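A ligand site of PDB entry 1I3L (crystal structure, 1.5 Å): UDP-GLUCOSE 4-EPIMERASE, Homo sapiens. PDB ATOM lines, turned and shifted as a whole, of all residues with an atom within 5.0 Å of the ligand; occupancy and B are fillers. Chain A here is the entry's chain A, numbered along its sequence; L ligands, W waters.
O6 of the ligand is in hydrogen-bond range of OD2 of Asp 33 (2.7 Å).
O13 of the ligand is in hydrogen-bond range of OH of Tyr 157 (2.7 Å).
An oxygen (O6) of the ligand is in hydrogen-bond range of the backbone NH (N) of Asn 37, 2.8 Å away.
The side-chain amide nitrogen (ND2) of Asn 37 sits at hydrogen-bond distance from an oxygen (O2) of the ligand.
OD1 of Asp 66 is in hydrogen-bond range of N3 of the ligand (2.8 Å).
The backbone NH (N) of Ile 14 sits at hydrogen-bond distance from an oxygen (O9) of the ligand (2.9 Å).
The side-chain amino group (NZ) of Lys 161 sits at hydrogen-bond distance from an oxygen (O12) of the ligand, at 2.9 Å.
N of Tyr 13 is in hydrogen-bond range of O1 of the ligand, 2.9 Å away.
O of Phe 88 is in hydrogen-bond range of O12 of the ligand (2.9 Å).
An oxygen (O8) of the ligand lies within salt-bridge range of the side-chain amino group (NZ) of Lys 92, at 2.9 Å.
An oxygen (O6) of the ligand is in hydrogen-bond range of the backbone NH (N) of His 36 (3.0 Å).
N of Asn 34 lies within hydrogen-bond range of N5 of the ligand (3.5 Å).
OD1 of Asn 34 lies close to N5 of the ligand (3.3 Å).
The backbone NH of Ile 67 sits at hydrogen-bond distance from a nitrogen (N4) of the ligand.
The backbone NH (N) of Gly 12 lies within hydrogen-bond range of an oxygen (O5) of the ligand.
The side-chain carboxylate (OD2) of Asp 33 lies within hydrogen-bond range of the backbone NH (N) of Phe 35 (2.8 Å).
The backbone NH (N) of Ala 11 is in hydrogen-bond range of the side-chain carboxylate (OD1) of Asp 33, 3.0 Å away.
N of Leu 68 sits at hydrogen-bond distance from OD1 of Asp 66 (2.7 Å).
NZ of Lys 161 sits at hydrogen-bond distance from O of Ser 130.
The side-chain amide oxygen (OD1) of Asn 34 lies within hydrogen-bond range of the backbone NH (N) of His 36.
The backbone NH (N) of Asn 34 lies within hydrogen-bond range of the backbone carbonyl oxygen (O) of Met 65 (3.4 Å).
OH of Tyr 185 lies within hydrogen-bond range of OG of Ser 130.
The backbone carbonyl oxygen of Ile 32 is in hydrogen-bond range of the backbone NH of Gly 9.
Gly 9 touches the ligand.
Ala 11 touches the ligand.
Phe 35 touches the ligand (C to O6, 3.6 Å).
Ala 38 touches the ligand.
Met 65 touches the ligand (O to C9, 3.6 Å).
Ala 89 touches the ligand (CB to N5, 3.6 Å).
Gly 90 touches the ligand.
CG1 of Val 107 touches N3 of the ligand, 3.7 Å away.
CB of Ser 130 touches O11 of the ligand, at 3.5 Å.
Ser 131 touches the ligand.
CB of Ser 132 touches C20 of the ligand (3.5 Å).
Tyr 185 touches the ligand.
Phe 186 touches the ligand.
CD of Pro 188 touches O14 of the ligand, 2.9 Å away.
Hydrophobic or aromatic side chains within 4 Å of the ligand: Tyr 13, Ile 14, His 36, Ala 38, Ile 67, Ala 89, Val 107, Tyr 157, Tyr 185 and Pro 188.
Of the 32 residues printed, 27 come within 4 Å of the ligand.
The nearest printed residue that does not touch the ligand is Gly 15 (4.2 Å).
Water W3 lies within hydrogen-bond range of O of Asn 37 and O1 of the ligand.
Water W6 lies within hydrogen-bond range of OD2 of Asp 66 (2.8 Å) and N3 of the ligand (2.9 Å).
Water W9 lies within hydrogen-bond range of the backbone carbonyl oxygen of Gly 90 (2.8 Å) and an oxygen (O2) of the ligand (2.9 Å).
Water W4 lies within hydrogen-bond range of the backbone carbonyl oxygen of Leu 91 (2.8 Å), an oxygen (O13) of the ligand (3.0 Å) and the side-chain amino group of Lys 161 (3.2 Å).
Water W2 lies within hydrogen-bond range of the backbone carbonyl oxygen of Ala 89 (2.9 Å), an oxygen (O12) of the ligand (3.1 Å), the backbone carbonyl oxygen of Phe 88 (3.3 Å) and the side-chain amino group of Lys 161 (3.4 Å).
Water W1 lies within hydrogen-bond range of the side-chain hydroxyl (OG) of Ser 132 and the side-chain hydroxyl (OH) of Tyr 157.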
ATOM      1  N   GLY A   9      -7.782  -5.533   1.749  1.00  0.00           N
ATOM      2  CA  GLY A   9      -8.636  -6.405   2.545  1.00  0.00           C
ATOM      3  C   GLY A   9      -9.034  -7.623   1.724  1.00  0.00           C
ATOM      4  O   GLY A   9     -10.072  -8.217   1.953  1.00  0.00           O
ATOM      5  N   ALA A  11      -8.130 -10.691   1.710  1.00  0.00           N
ATOM      6  CA  ALA A  11      -8.181 -12.039   2.251  1.00  0.00           C
ATOM      7  C   ALA A  11      -9.496 -12.369   2.954  1.00  0.00           C
ATOM      8  O   ALA A  11      -9.733 -13.527   3.316  1.00  0.00           O
ATOM      9  CB  ALA A  11      -7.067 -12.183   3.269  1.00  0.00           C
ATOM     10  N   GLY A  12     -10.350 -11.348   3.175  1.00  0.00           N
ATOM     11  CA  GLY A  12     -11.615 -11.503   3.878  1.00  0.00           C
ATOM     12  C   GLY A  12     -12.674 -12.198   3.042  1.00  0.00           C
ATOM     13  O   GLY A  12     -12.431 -12.703   1.959  1.00  0.00           O
ATOM     14  N   TYR A  13     -13.893 -12.138   3.573  1.00  0.00           N
ATOM     15  CA  TYR A  13     -15.035 -12.787   2.938  1.00  0.00           C
ATOM     16  C   TYR A  13     -15.333 -12.357   1.523  1.00  0.00           C
ATOM     17  O   TYR A  13     -15.245 -13.109   0.541  1.00  0.00           O
ATOM     18  CB  TYR A  13     -16.221 -12.646   3.887  1.00  0.00           C
ATOM     19  CG  TYR A  13     -17.467 -13.289   3.380  1.00  0.00           C
ATOM     20  CD1 TYR A  13     -17.480 -14.476   2.638  1.00  0.00           C
ATOM     21  CD2 TYR A  13     -18.687 -12.696   3.694  1.00  0.00           C
ATOM     22  CE1 TYR A  13     -18.679 -15.036   2.191  1.00  0.00           C
ATOM     23  CE2 TYR A  13     -19.887 -13.254   3.257  1.00  0.00           C
ATOM     24  CZ  TYR A  13     -19.893 -14.433   2.513  1.00  0.00           C
ATOM     25  OH  TYR A  13     -21.109 -14.982   2.104  1.00  0.00           O
ATOM     26  N   ILE A  14     -15.726 -11.076   1.395  1.00  0.00           N
ATOM     27  CA  ILE A  14     -16.050 -10.557   0.077  1.00  0.00           C
ATOM     28  C   ILE A  14     -14.842 -10.399  -0.810  1.00  0.00           C
ATOM     29  O   ILE A  14     -14.863 -10.673  -2.018  1.00  0.00           O
ATOM     30  CB  ILE A  14     -16.882  -9.244   0.183  1.00  0.00           C
ATOM     31  CG1 ILE A  14     -18.086  -9.469   1.092  1.00  0.00           C
ATOM     32  CG2 ILE A  14     -17.332  -8.795  -1.206  1.00  0.00           C
ATOM     33  CD1 ILE A  14     -18.807  -8.201   1.557  1.00  0.00           C
ATOM     34  N   GLY A  15     -13.740  -9.941  -0.200  1.00  0.00           N
ATOM     35  CA  GLY A  15     -12.492  -9.736  -0.930  1.00  0.00           C
ATOM     36  C   GLY A  15     -11.947 -11.015  -1.573  1.00  0.00           C
ATOM     37  O   GLY A  15     -11.554 -11.004  -2.730  1.00  0.00           O
ATOM     38  N   ILE A  32      -3.605  -6.940  -0.640  1.00  0.00           N
ATOM     39  CA  ILE A  32      -3.016  -6.623   0.645  1.00  0.00           C
ATOM     40  C   ILE A  32      -4.017  -6.898   1.742  1.00  0.00           C
ATOM     41  O   ILE A  32      -5.225  -6.712   1.547  1.00  0.00           O
ATOM     42  CB  ILE A  32      -2.430  -5.218   0.796  1.00  0.00           C
ATOM     43  CG1 ILE A  32      -3.536  -4.175   0.708  1.00  0.00           C
ATOM     44  CG2 ILE A  32      -1.337  -4.894  -0.216  1.00  0.00           C
ATOM     45  CD1 ILE A  32      -2.973  -2.764   0.908  1.00  0.00           C
ATOM     46  N   ASP A  33      -3.534  -7.297   2.916  1.00  0.00           N
ATOM     47  CA  ASP A  33      -4.373  -7.590   4.083  1.00  0.00           C
ATOM     48  C   ASP A  33      -3.459  -7.642   5.289  1.00  0.00           C
ATOM     49  O   ASP A  33      -2.305  -8.018   5.100  1.00  0.00           O
ATOM     50  CB  ASP A  33      -5.150  -8.934   3.931  1.00  0.00           C
ATOM     51  CG  ASP A  33      -6.436  -9.028   4.686  1.00  0.00           C
ATOM     52  OD1 ASP A  33      -7.513  -9.026   4.086  1.00  0.00           O
ATOM     53  OD2 ASP A  33      -6.327  -9.094   6.001  1.00  0.00           O
ATOM     54  N   ASN A  34      -3.957  -7.267   6.461  1.00  0.00           N
ATOM     55  CA  ASN A  34      -3.174  -7.277   7.687  1.00  0.00           C
ATOM     56  C   ASN A  34      -3.610  -8.377   8.628  1.00  0.00           C
ATOM     57  O   ASN A  34      -3.175  -8.441   9.764  1.00  0.00           O
ATOM     58  CB  ASN A  34      -3.268  -5.925   8.431  1.00  0.00           C
ATOM     59  CG  ASN A  34      -4.642  -5.663   9.044  1.00  0.00           C
ATOM     60  OD1 ASN A  34      -5.620  -6.415   8.780  1.00  0.00           O
ATOM     61  ND2 ASN A  34      -4.736  -4.611   9.896  1.00  0.00           N
ATOM     62  N   PHE A  35      -4.477  -9.247   8.146  1.00  0.00           N
ATOM     63  CA  PHE A  35      -4.927 -10.369   8.956  1.00  0.00           C
ATOM     64  C   PHE A  35      -5.780  -9.998  10.148  1.00  0.00           C
ATOM     65  O   PHE A  35      -5.968 -10.809  11.053  1.00  0.00           O
ATOM     66  CB  PHE A  35      -3.714 -11.246   9.408  1.00  0.00           C
ATOM     67  CG  PHE A  35      -3.088 -11.961   8.219  1.00  0.00           C
ATOM     68  CD1 PHE A  35      -1.866 -11.605   7.658  1.00  0.00           C
ATOM     69  CD2 PHE A  35      -3.769 -13.048   7.652  1.00  0.00           C
ATOM     70  CE1 PHE A  35      -1.312 -12.272   6.564  1.00  0.00           C
ATOM     71  CE2 PHE A  35      -3.235 -13.736   6.563  1.00  0.00           C
ATOM     72  CZ  PHE A  35      -2.009 -13.353   6.015  1.00  0.00           C
ATOM     73  N   HIS A  36      -6.308  -8.788  10.171  1.00  0.00           N
ATOM     74  CA  HIS A  36      -7.137  -8.407  11.276  1.00  0.00           C
ATOM     75  C   HIS A  36      -8.314  -9.349  11.430  1.00  0.00           C
ATOM     76  O   HIS A  36      -8.735  -9.692  12.536  1.00  0.00           O
ATOM     77  CB  HIS A  36      -7.610  -6.934  11.134  1.00  0.00           C
ATOM     78  CG  HIS A  36      -8.601  -6.535  12.169  1.00  0.00           C
ATOM     79  ND1 HIS A  36      -8.214  -6.185  13.462  1.00  0.00           N
ATOM     80  CD2 HIS A  36      -9.971  -6.418  12.092  1.00  0.00           C
ATOM     81  CE1 HIS A  36      -9.331  -5.878  14.130  1.00  0.00           C
ATOM     82  NE2 HIS A  36     -10.410  -6.020  13.344  1.00  0.00           N
ATOM     83  N   ASN A  37      -8.861  -9.746  10.300  1.00  0.00           N
ATOM     84  CA  ASN A  37     -10.016 -10.641  10.345  1.00  0.00           C
ATOM     85  C   ASN A  37      -9.948 -11.683   9.235  1.00  0.00           C
ATOM     86  O   ASN A  37     -10.942 -11.946   8.537  1.00  0.00           O
ATOM     87  CB  ASN A  37     -11.359  -9.833  10.275  1.00  0.00           C
ATOM     88  CG  ASN A  37     -12.594 -10.660  10.567  1.00  0.00           C
ATOM     89  OD1 ASN A  37     -12.597 -11.496  11.493  1.00  0.00           O
ATOM     90  ND2 ASN A  37     -13.670 -10.424   9.816  1.00  0.00           N
ATOM     91  N   ALA A  38      -8.759 -12.227   9.050  1.00  0.00           N
ATOM     92  CA  ALA A  38      -8.477 -13.243   8.040  1.00  0.00           C
ATOM     93  C   ALA A  38      -7.462 -14.204   8.643  1.00  0.00           C
ATOM     94  O   ALA A  38      -6.568 -13.793   9.402  1.00  0.00           O
ATOM     95  CB  ALA A  38      -7.996 -12.669   6.716  1.00  0.00           C
ATOM     96  N   MET A  65       0.122  -6.339   4.833  1.00  0.00           N
ATOM     97  CA  MET A  65       0.342  -4.926   5.062  1.00  0.00           C
ATOM     98  C   MET A  65      -0.899  -4.277   5.620  1.00  0.00           C
ATOM     99  O   MET A  65      -2.007  -4.739   5.337  1.00  0.00           O
ATOM    100  CB  MET A  65       0.635  -4.354   3.662  1.00  0.00           C
ATOM    101  CG  MET A  65       0.744  -2.841   3.630  1.00  0.00           C
ATOM    102  SD  MET A  65       0.971  -2.198   1.960  1.00  0.00           S
ATOM    103  CE  MET A  65       2.319  -3.266   1.377  1.00  0.00           C
ATOM    104  N   ASP A  66      -0.713  -3.213   6.382  1.00  0.00           N
ATOM    105  CA  ASP A  66      -1.822  -2.462   6.948  1.00  0.00           C
ATOM    106  C   ASP A  66      -2.023  -1.191   6.140  1.00  0.00           C
ATOM    107  O   ASP A  66      -1.064  -0.509   5.762  1.00  0.00           O
ATOM    108  CB  ASP A  66      -1.527  -2.100   8.388  1.00  0.00           C
ATOM    109  CG  ASP A  66      -2.703  -1.548   9.109  1.00  0.00           C
ATOM    110  OD1 ASP A  66      -3.477  -0.735   8.665  1.00  0.00           O
ATOM    111  OD2 ASP A  66      -2.826  -2.085  10.288  1.00  0.00           O
ATOM    112  N   ILE A  67      -3.278  -0.825   5.842  1.00  0.00           N
ATOM    113  CA  ILE A  67      -3.497   0.387   5.063  1.00  0.00           C
ATOM    114  C   ILE A  67      -3.077   1.614   5.840  1.00  0.00           C
ATOM    115  O   ILE A  67      -2.893   2.676   5.243  1.00  0.00           O
ATOM    116  CB  ILE A  67      -4.947   0.633   4.579  1.00  0.00           C
ATOM    117  CG1 ILE A  67      -5.875   0.696   5.803  1.00  0.00           C
ATOM    118  CG2 ILE A  67      -5.319  -0.479   3.620  1.00  0.00           C
ATOM    119  CD1 ILE A  67      -7.319   1.052   5.494  1.00  0.00           C
ATOM    120  N   LEU A  68      -2.932   1.461   7.154  1.00  0.00           N
ATOM    121  CA  LEU A  68      -2.497   2.575   7.969  1.00  0.00           C
ATOM    122  C   LEU A  68      -0.987   2.784   7.940  1.00  0.00           C
ATOM    123  O   LEU A  68      -0.509   3.780   8.459  1.00  0.00           O
ATOM    124  CB  LEU A  68      -2.971   2.441   9.425  1.00  0.00           C
ATOM    125  CG  LEU A  68      -4.495   2.499   9.587  1.00  0.00           C
ATOM    126  CD1 LEU A  68      -4.763   2.122  11.031  1.00  0.00           C
ATOM    127  CD2 LEU A  68      -5.030   3.911   9.365  1.00  0.00           C
ATOM    128  N   PHE A  88     -11.628  -2.997   0.104  1.00  0.00           N
ATOM    129  CA  PHE A  88     -12.428  -3.757   1.088  1.00  0.00           C
ATOM    130  C   PHE A  88     -11.938  -3.599   2.524  1.00  0.00           C
ATOM    131  O   PHE A  88     -12.675  -3.839   3.512  1.00  0.00           O
ATOM    132  CB  PHE A  88     -12.381  -5.287   0.810  1.00  0.00           C
ATOM    133  CG  PHE A  88     -13.038  -5.723  -0.483  1.00  0.00           C
ATOM    134  CD1 PHE A  88     -14.422  -5.858  -0.575  1.00  0.00           C
ATOM    135  CD2 PHE A  88     -12.276  -6.060  -1.597  1.00  0.00           C
ATOM    136  CE1 PHE A  88     -15.037  -6.250  -1.764  1.00  0.00           C
ATOM    137  CE2 PHE A  88     -12.875  -6.481  -2.786  1.00  0.00           C
ATOM    138  CZ  PHE A  88     -14.257  -6.549  -2.879  1.00  0.00           C
ATOM    139  N   ALA A  89     -10.652  -3.252   2.667  1.00  0.00           N
ATOM    140  CA  ALA A  89     -10.109  -3.161   3.980  1.00  0.00           C
ATOM    141  C   ALA A  89     -10.807  -2.229   4.915  1.00  0.00           C
ATOM    142  O   ALA A  89     -11.034  -1.053   4.591  1.00  0.00           O
ATOM    143  CB  ALA A  89      -8.610  -2.826   3.973  1.00  0.00           C
ATOM    144  N   GLY A  90     -11.104  -2.728   6.112  1.00  0.00           N
ATOM    145  CA  GLY A  90     -11.738  -1.933   7.159  1.00  0.00           C
ATOM    146  C   GLY A  90     -12.255  -2.767   8.313  1.00  0.00           C
ATOM    147  O   GLY A  90     -12.177  -4.018   8.262  1.00  0.00           O
ATOM    148  N   LEU A  91     -12.801  -2.075   9.326  1.00  0.00           N
ATOM    149  CA  LEU A  91     -13.400  -2.759  10.457  1.00  0.00           C
ATOM    150  C   LEU A  91     -14.884  -2.808  10.193  1.00  0.00           C
ATOM    151  O   LEU A  91     -15.462  -1.856   9.697  1.00  0.00           O
ATOM    152  CB  LEU A  91     -13.262  -1.996  11.788  1.00  0.00           C
ATOM    153  CG  LEU A  91     -11.834  -1.710  12.234  1.00  0.00           C
ATOM    154  CD1 LEU A  91     -11.925  -1.122  13.627  1.00  0.00           C
ATOM    155  CD2 LEU A  91     -10.960  -2.974  12.199  1.00  0.00           C
ATOM    156  N   LYS A  92     -15.499  -3.935  10.529  1.00  0.00           N
ATOM    157  CA  LYS A  92     -16.925  -4.049  10.375  1.00  0.00           C
ATOM    158  C   LYS A  92     -17.386  -4.294  11.763  1.00  0.00           C
ATOM    159  O   LYS A  92     -16.594  -4.291  12.711  1.00  0.00           O
ATOM    160  CB  LYS A  92     -17.523  -4.975   9.351  1.00  0.00           C
ATOM    161  CG  LYS A  92     -16.650  -6.130   8.943  1.00  0.00           C
ATOM    162  CD  LYS A  92     -17.419  -7.169   8.155  1.00  0.00           C
ATOM    163  CE  LYS A  92     -17.199  -8.596   8.645  1.00  0.00           C
ATOM    164  NZ  LYS A  92     -17.989  -9.557   7.872  1.00  0.00           N
ATOM    165  N   VAL A 107      -9.298   3.287  11.546  1.00  0.00           N
ATOM    166  CA  VAL A 107      -9.146   2.318  10.481  1.00  0.00           C
ATOM    167  C   VAL A 107      -9.955   2.640   9.257  1.00  0.00           C
ATOM    168  O   VAL A 107      -9.412   2.619   8.173  1.00  0.00           O
ATOM    169  CB  VAL A 107      -9.426   0.873  10.912  1.00  0.00           C
ATOM    170  CG1 VAL A 107      -9.144  -0.062   9.739  1.00  0.00           C
ATOM    171  CG2 VAL A 107      -8.490   0.500  12.066  1.00  0.00           C
ATOM    172  N   SER A 130     -16.126  -0.277  -0.896  1.00  0.00           N
ATOM    173  CA  SER A 130     -17.114  -1.101  -0.220  1.00  0.00           C
ATOM    174  C   SER A 130     -17.974  -0.281   0.729  1.00  0.00           C
ATOM    175  O   SER A 130     -17.590   0.026   1.846  1.00  0.00           O
ATOM    176  CB  SER A 130     -16.429  -2.159   0.656  1.00  0.00           C
ATOM    177  OG  SER A 130     -15.671  -3.005  -0.166  1.00  0.00           O
ATOM    178  N   SER A 131     -19.172   0.069   0.303  1.00  0.00           N
ATOM    179  CA  SER A 131     -20.104   0.809   1.116  1.00  0.00           C
ATOM    180  C   SER A 131     -21.189  -0.143   1.648  1.00  0.00           C
ATOM    181  O   SER A 131     -21.102  -1.364   1.482  1.00  0.00           O
ATOM    182  CB  SER A 131     -20.684   2.043   0.432  1.00  0.00           C
ATOM    183  OG  SER A 131     -21.281   2.824   1.455  1.00  0.00           O
ATOM    184  N   SER A 132     -22.231   0.381   2.260  1.00  0.00           N
ATOM    185  CA  SER A 132     -23.232  -0.488   2.824  1.00  0.00           C
ATOM    186  C   SER A 132     -24.597   0.174   2.906  1.00  0.00           C
ATOM    187  O   SER A 132     -24.710   1.377   3.022  1.00  0.00           O
ATOM    188  CB  SER A 132     -22.768  -0.774   4.255  1.00  0.00           C
ATOM    189  OG  SER A 132     -23.822  -1.166   5.144  1.00  0.00           O
ATOM    190  N   TYR A 157     -19.830   2.649  12.876  1.00  0.00           N
ATOM    191  CA  TYR A 157     -19.459   1.940  11.667  1.00  0.00           C
ATOM    192  C   TYR A 157     -20.163   2.538  10.445  1.00  0.00           C
ATOM    193  O   TYR A 157     -19.567   2.795   9.400  1.00  0.00           O
ATOM    194  CB  TYR A 157     -19.852   0.452  11.810  1.00  0.00           C
ATOM    195  CG  TYR A 157     -19.803  -0.249  10.471  1.00  0.00           C
ATOM    196  CD1 TYR A 157     -20.993  -0.570   9.821  1.00  0.00           C
ATOM    197  CD2 TYR A 157     -18.606  -0.589   9.841  1.00  0.00           C
ATOM    198  CE1 TYR A 157     -20.975  -1.202   8.584  1.00  0.00           C
ATOM    199  CE2 TYR A 157     -18.565  -1.243   8.602  1.00  0.00           C
ATOM    200  CZ  TYR A 157     -19.764  -1.562   7.982  1.00  0.00           C
ATOM    201  OH  TYR A 157     -19.783  -2.194   6.774  1.00  0.00           O
ATOM    202  N   LYS A 161     -18.793   4.836   7.101  1.00  0.00           N
ATOM    203  CA  LYS A 161     -19.035   4.564   5.719  1.00  0.00           C
ATOM    204  C   LYS A 161     -19.629   5.796   5.035  1.00  0.00           C
ATOM    205  O   LYS A 161     -19.270   6.134   3.905  1.00  0.00           O
ATOM    206  CB  LYS A 161     -19.917   3.322   5.537  1.00  0.00           C
ATOM    207  CG  LYS A 161     -19.233   2.000   5.930  1.00  0.00           C
ATOM    208  CD  LYS A 161     -18.069   1.599   5.011  1.00  0.00           C
ATOM    209  CE  LYS A 161     -17.655   0.110   5.050  1.00  0.00           C
ATOM    210  NZ  LYS A 161     -16.379  -0.115   4.345  1.00  0.00           N
ATOM    211  N   TYR A 185     -23.394  -2.449  -0.363  1.00  0.00           N
ATOM    212  CA  TYR A 185     -23.857  -3.822  -0.285  1.00  0.00           C
ATOM    213  C   TYR A 185     -25.031  -4.005   0.676  1.00  0.00           C
ATOM    214  O   TYR A 185     -25.167  -3.277   1.663  1.00  0.00           O
ATOM    215  CB  TYR A 185     -22.751  -4.750   0.282  1.00  0.00           C
ATOM    216  CG  TYR A 185     -21.337  -4.582  -0.278  1.00  0.00           C
ATOM    217  CD1 TYR A 185     -21.105  -4.167  -1.599  1.00  0.00           C
ATOM    218  CD2 TYR A 185     -20.242  -4.902   0.533  1.00  0.00           C
ATOM    219  CE1 TYR A 185     -19.816  -4.054  -2.118  1.00  0.00           C
ATOM    220  CE2 TYR A 185     -18.954  -4.782   0.033  1.00  0.00           C
ATOM    221  CZ  TYR A 185     -18.739  -4.335  -1.279  1.00  0.00           C
ATOM    222  OH  TYR A 185     -17.447  -4.206  -1.729  1.00  0.00           O
ATOM    223  N   PHE A 186     -25.873  -5.017   0.411  1.00  0.00           N
ATOM    224  CA  PHE A 186     -26.957  -5.322   1.323  1.00  0.00           C
ATOM    225  C   PHE A 186     -26.479  -6.403   2.287  1.00  0.00           C
ATOM    226  O   PHE A 186     -25.529  -6.137   3.002  1.00  0.00           O
ATOM    227  CB  PHE A 186     -28.300  -5.571   0.628  1.00  0.00           C
ATOM    228  CG  PHE A 186     -28.891  -4.203   0.311  1.00  0.00           C
ATOM    229  CD1 PHE A 186     -30.046  -3.785   0.961  1.00  0.00           C
ATOM    230  CD2 PHE A 186     -28.260  -3.337  -0.592  1.00  0.00           C
ATOM    231  CE1 PHE A 186     -30.569  -2.513   0.722  1.00  0.00           C
ATOM    232  CE2 PHE A 186     -28.782  -2.071  -0.851  1.00  0.00           C
ATOM    233  CZ  PHE A 186     -29.936  -1.664  -0.187  1.00  0.00           C
ATOM    234  N   ASN A 187     -27.055  -7.600   2.332  1.00  0.00           N
ATOM    235  CA  ASN A 187     -26.588  -8.645   3.295  1.00  0.00           C
ATOM    236  C   ASN A 187     -25.920  -9.821   2.574  1.00  0.00           C
ATOM    237  O   ASN A 187     -26.576 -10.789   2.181  1.00  0.00           O
ATOM    238  CB  ASN A 187     -27.759  -9.143   4.158  1.00  0.00           C
ATOM    239  CG  ASN A 187     -28.152  -8.073   5.153  1.00  0.00           C
ATOM    240  OD1 ASN A 187     -28.518  -6.978   4.729  1.00  0.00           O
ATOM    241  ND2 ASN A 187     -28.005  -8.329   6.447  1.00  0.00           N
ATOM    242  N   PRO A 188     -24.604  -9.739   2.341  1.00  0.00           N
ATOM    243  CA  PRO A 188     -23.924 -10.817   1.621  1.00  0.00           C
ATOM    244  C   PRO A 188     -23.969 -12.158   2.361  1.00  0.00           C
ATOM    245  O   PRO A 188     -23.755 -12.239   3.561  1.00  0.00           O
ATOM    246  CB  PRO A 188     -22.457 -10.376   1.492  1.00  0.00           C
ATOM    247  CG  PRO A 188     -22.349  -8.994   2.103  1.00  0.00           C
ATOM    248  CD  PRO A 188     -23.652  -8.711   2.830  1.00  0.00           C
HETATM  249  P1  LIG L   1     -13.905  -9.051   6.276  1.00  0.00           P
HETATM  250  O1  LIG L   1     -13.933 -10.512   5.949  1.00  0.00           O
HETATM  251  O2  LIG L   1     -13.622  -8.681   7.650  1.00  0.00           O
HETATM  252  O3  LIG L   1     -12.946  -8.375   5.203  1.00  0.00           O
HETATM  253  C1  LIG L   1     -12.176  -7.182   5.488  1.00  0.00           C
HETATM  254  C2  LIG L   1     -10.701  -7.536   5.387  1.00  0.00           C
HETATM  255  O4  LIG L   1      -9.964  -6.337   5.742  1.00  0.00           O
HETATM  256  C3  LIG L   1     -10.210  -8.620   6.385  1.00  0.00           C
HETATM  257  O5  LIG L   1      -9.573  -9.709   5.687  1.00  0.00           O
HETATM  258  C4  LIG L   1      -9.315  -7.822   7.366  1.00  0.00           C
HETATM  259  O6  LIG L   1      -8.201  -8.624   7.819  1.00  0.00           O
HETATM  260  C5  LIG L   1      -8.834  -6.695   6.473  1.00  0.00           C
HETATM  261  N1  LIG L   1      -8.408  -5.504   7.188  1.00  0.00           N
HETATM  262  C6  LIG L   1      -9.012  -4.911   8.250  1.00  0.00           C
HETATM  263  N2  LIG L   1      -8.362  -3.815   8.696  1.00  0.00           N
HETATM  264  C7  LIG L   1      -7.292  -3.709   7.817  1.00  0.00           C
HETATM  265  C8  LIG L   1      -6.232  -2.762   7.748  1.00  0.00           C
HETATM  266  N3  LIG L   1      -6.108  -1.779   8.617  1.00  0.00           N
HETATM  267  N4  LIG L   1      -5.343  -2.956   6.723  1.00  0.00           N
HETATM  268  C9  LIG L   1      -5.490  -4.021   5.880  1.00  0.00           C
HETATM  269  N5  LIG L   1      -6.443  -4.945   5.885  1.00  0.00           N
HETATM  270  C10 LIG L   1      -7.303  -4.741   6.888  1.00  0.00           C
HETATM  271  O7  LIG L   1     -15.237  -8.312   5.882  1.00  0.00           O
HETATM  272  P2  LIG L   1     -16.184  -8.502   4.583  1.00  0.00           P
HETATM  273  O8  LIG L   1     -17.457  -9.117   5.025  1.00  0.00           O
HETATM  274  O9  LIG L   1     -15.452  -9.180   3.526  1.00  0.00           O
HETATM  275  O10 LIG L   1     -16.430  -6.947   4.281  1.00  0.00           O
HETATM  276  C11 LIG L   1     -15.606  -6.370   3.253  1.00  0.00           C
HETATM  277  C12 LIG L   1     -15.899  -4.882   3.212  1.00  0.00           C
HETATM  278  O11 LIG L   1     -17.295  -4.731   2.816  1.00  0.00           O
HETATM  279  C13 LIG L   1     -15.717  -4.124   4.516  1.00  0.00           C
HETATM  280  O12 LIG L   1     -15.247  -2.762   4.315  1.00  0.00           O
HETATM  281  C14 LIG L   1     -17.138  -4.122   5.073  1.00  0.00           C
HETATM  282  O13 LIG L   1     -17.303  -3.036   6.025  1.00  0.00           O
HETATM  283  C15 LIG L   1     -17.958  -3.981   3.802  1.00  0.00           C
HETATM  284  N6  LIG L   1     -19.354  -4.437   3.961  1.00  0.00           N
HETATM  285  C16 LIG L   1     -19.521  -5.761   4.350  1.00  0.00           C
HETATM  286  C17 LIG L   1     -20.808  -6.206   4.608  1.00  0.00           C
HETATM  287  C18 LIG L   1     -21.106  -7.627   5.072  1.00  0.00           C
HETATM  288  O14 LIG L   1     -22.274  -7.941   5.296  1.00  0.00           O
HETATM  289  N7  LIG L   1     -20.135  -8.538   5.245  1.00  0.00           N
HETATM  290  C19 LIG L   1     -21.933  -5.334   4.438  1.00  0.00           C
HETATM  291  C20 LIG L   1     -21.606  -4.026   4.013  1.00  0.00           C
HETATM  292  C21 LIG L   1     -20.373  -3.521   3.742  1.00  0.00           C
HETATM  293  O   HOH W   1     -22.958  -3.484   6.843  1.00  0.00           O
HETATM  294  O   HOH W   2     -13.361  -0.682   2.890  1.00  0.00           O
HETATM  295  O   HOH W   3     -12.672 -12.797   6.895  1.00  0.00           O
HETATM  296  O   HOH W   4     -15.093  -1.313   6.994  1.00  0.00           O
HETATM  297  O   HOH W   5     -23.790  -7.092   7.847  1.00  0.00           O
HETATM  298  O   HOH W   6      -5.338  -1.347  11.363  1.00  0.00           O
HETATM  299  O   HOH W   7      -7.186  -3.394  11.231  1.00  0.00           O
HETATM  300  O   HOH W   8     -13.017  -8.876   2.190  1.00  0.00           O
HETATM  301  O   HOH W   9     -12.328  -6.584   9.246  1.00  0.00           O
HETATM  302  O   HOH W  10     -15.234 -12.633   7.395  1.00  0.00           O
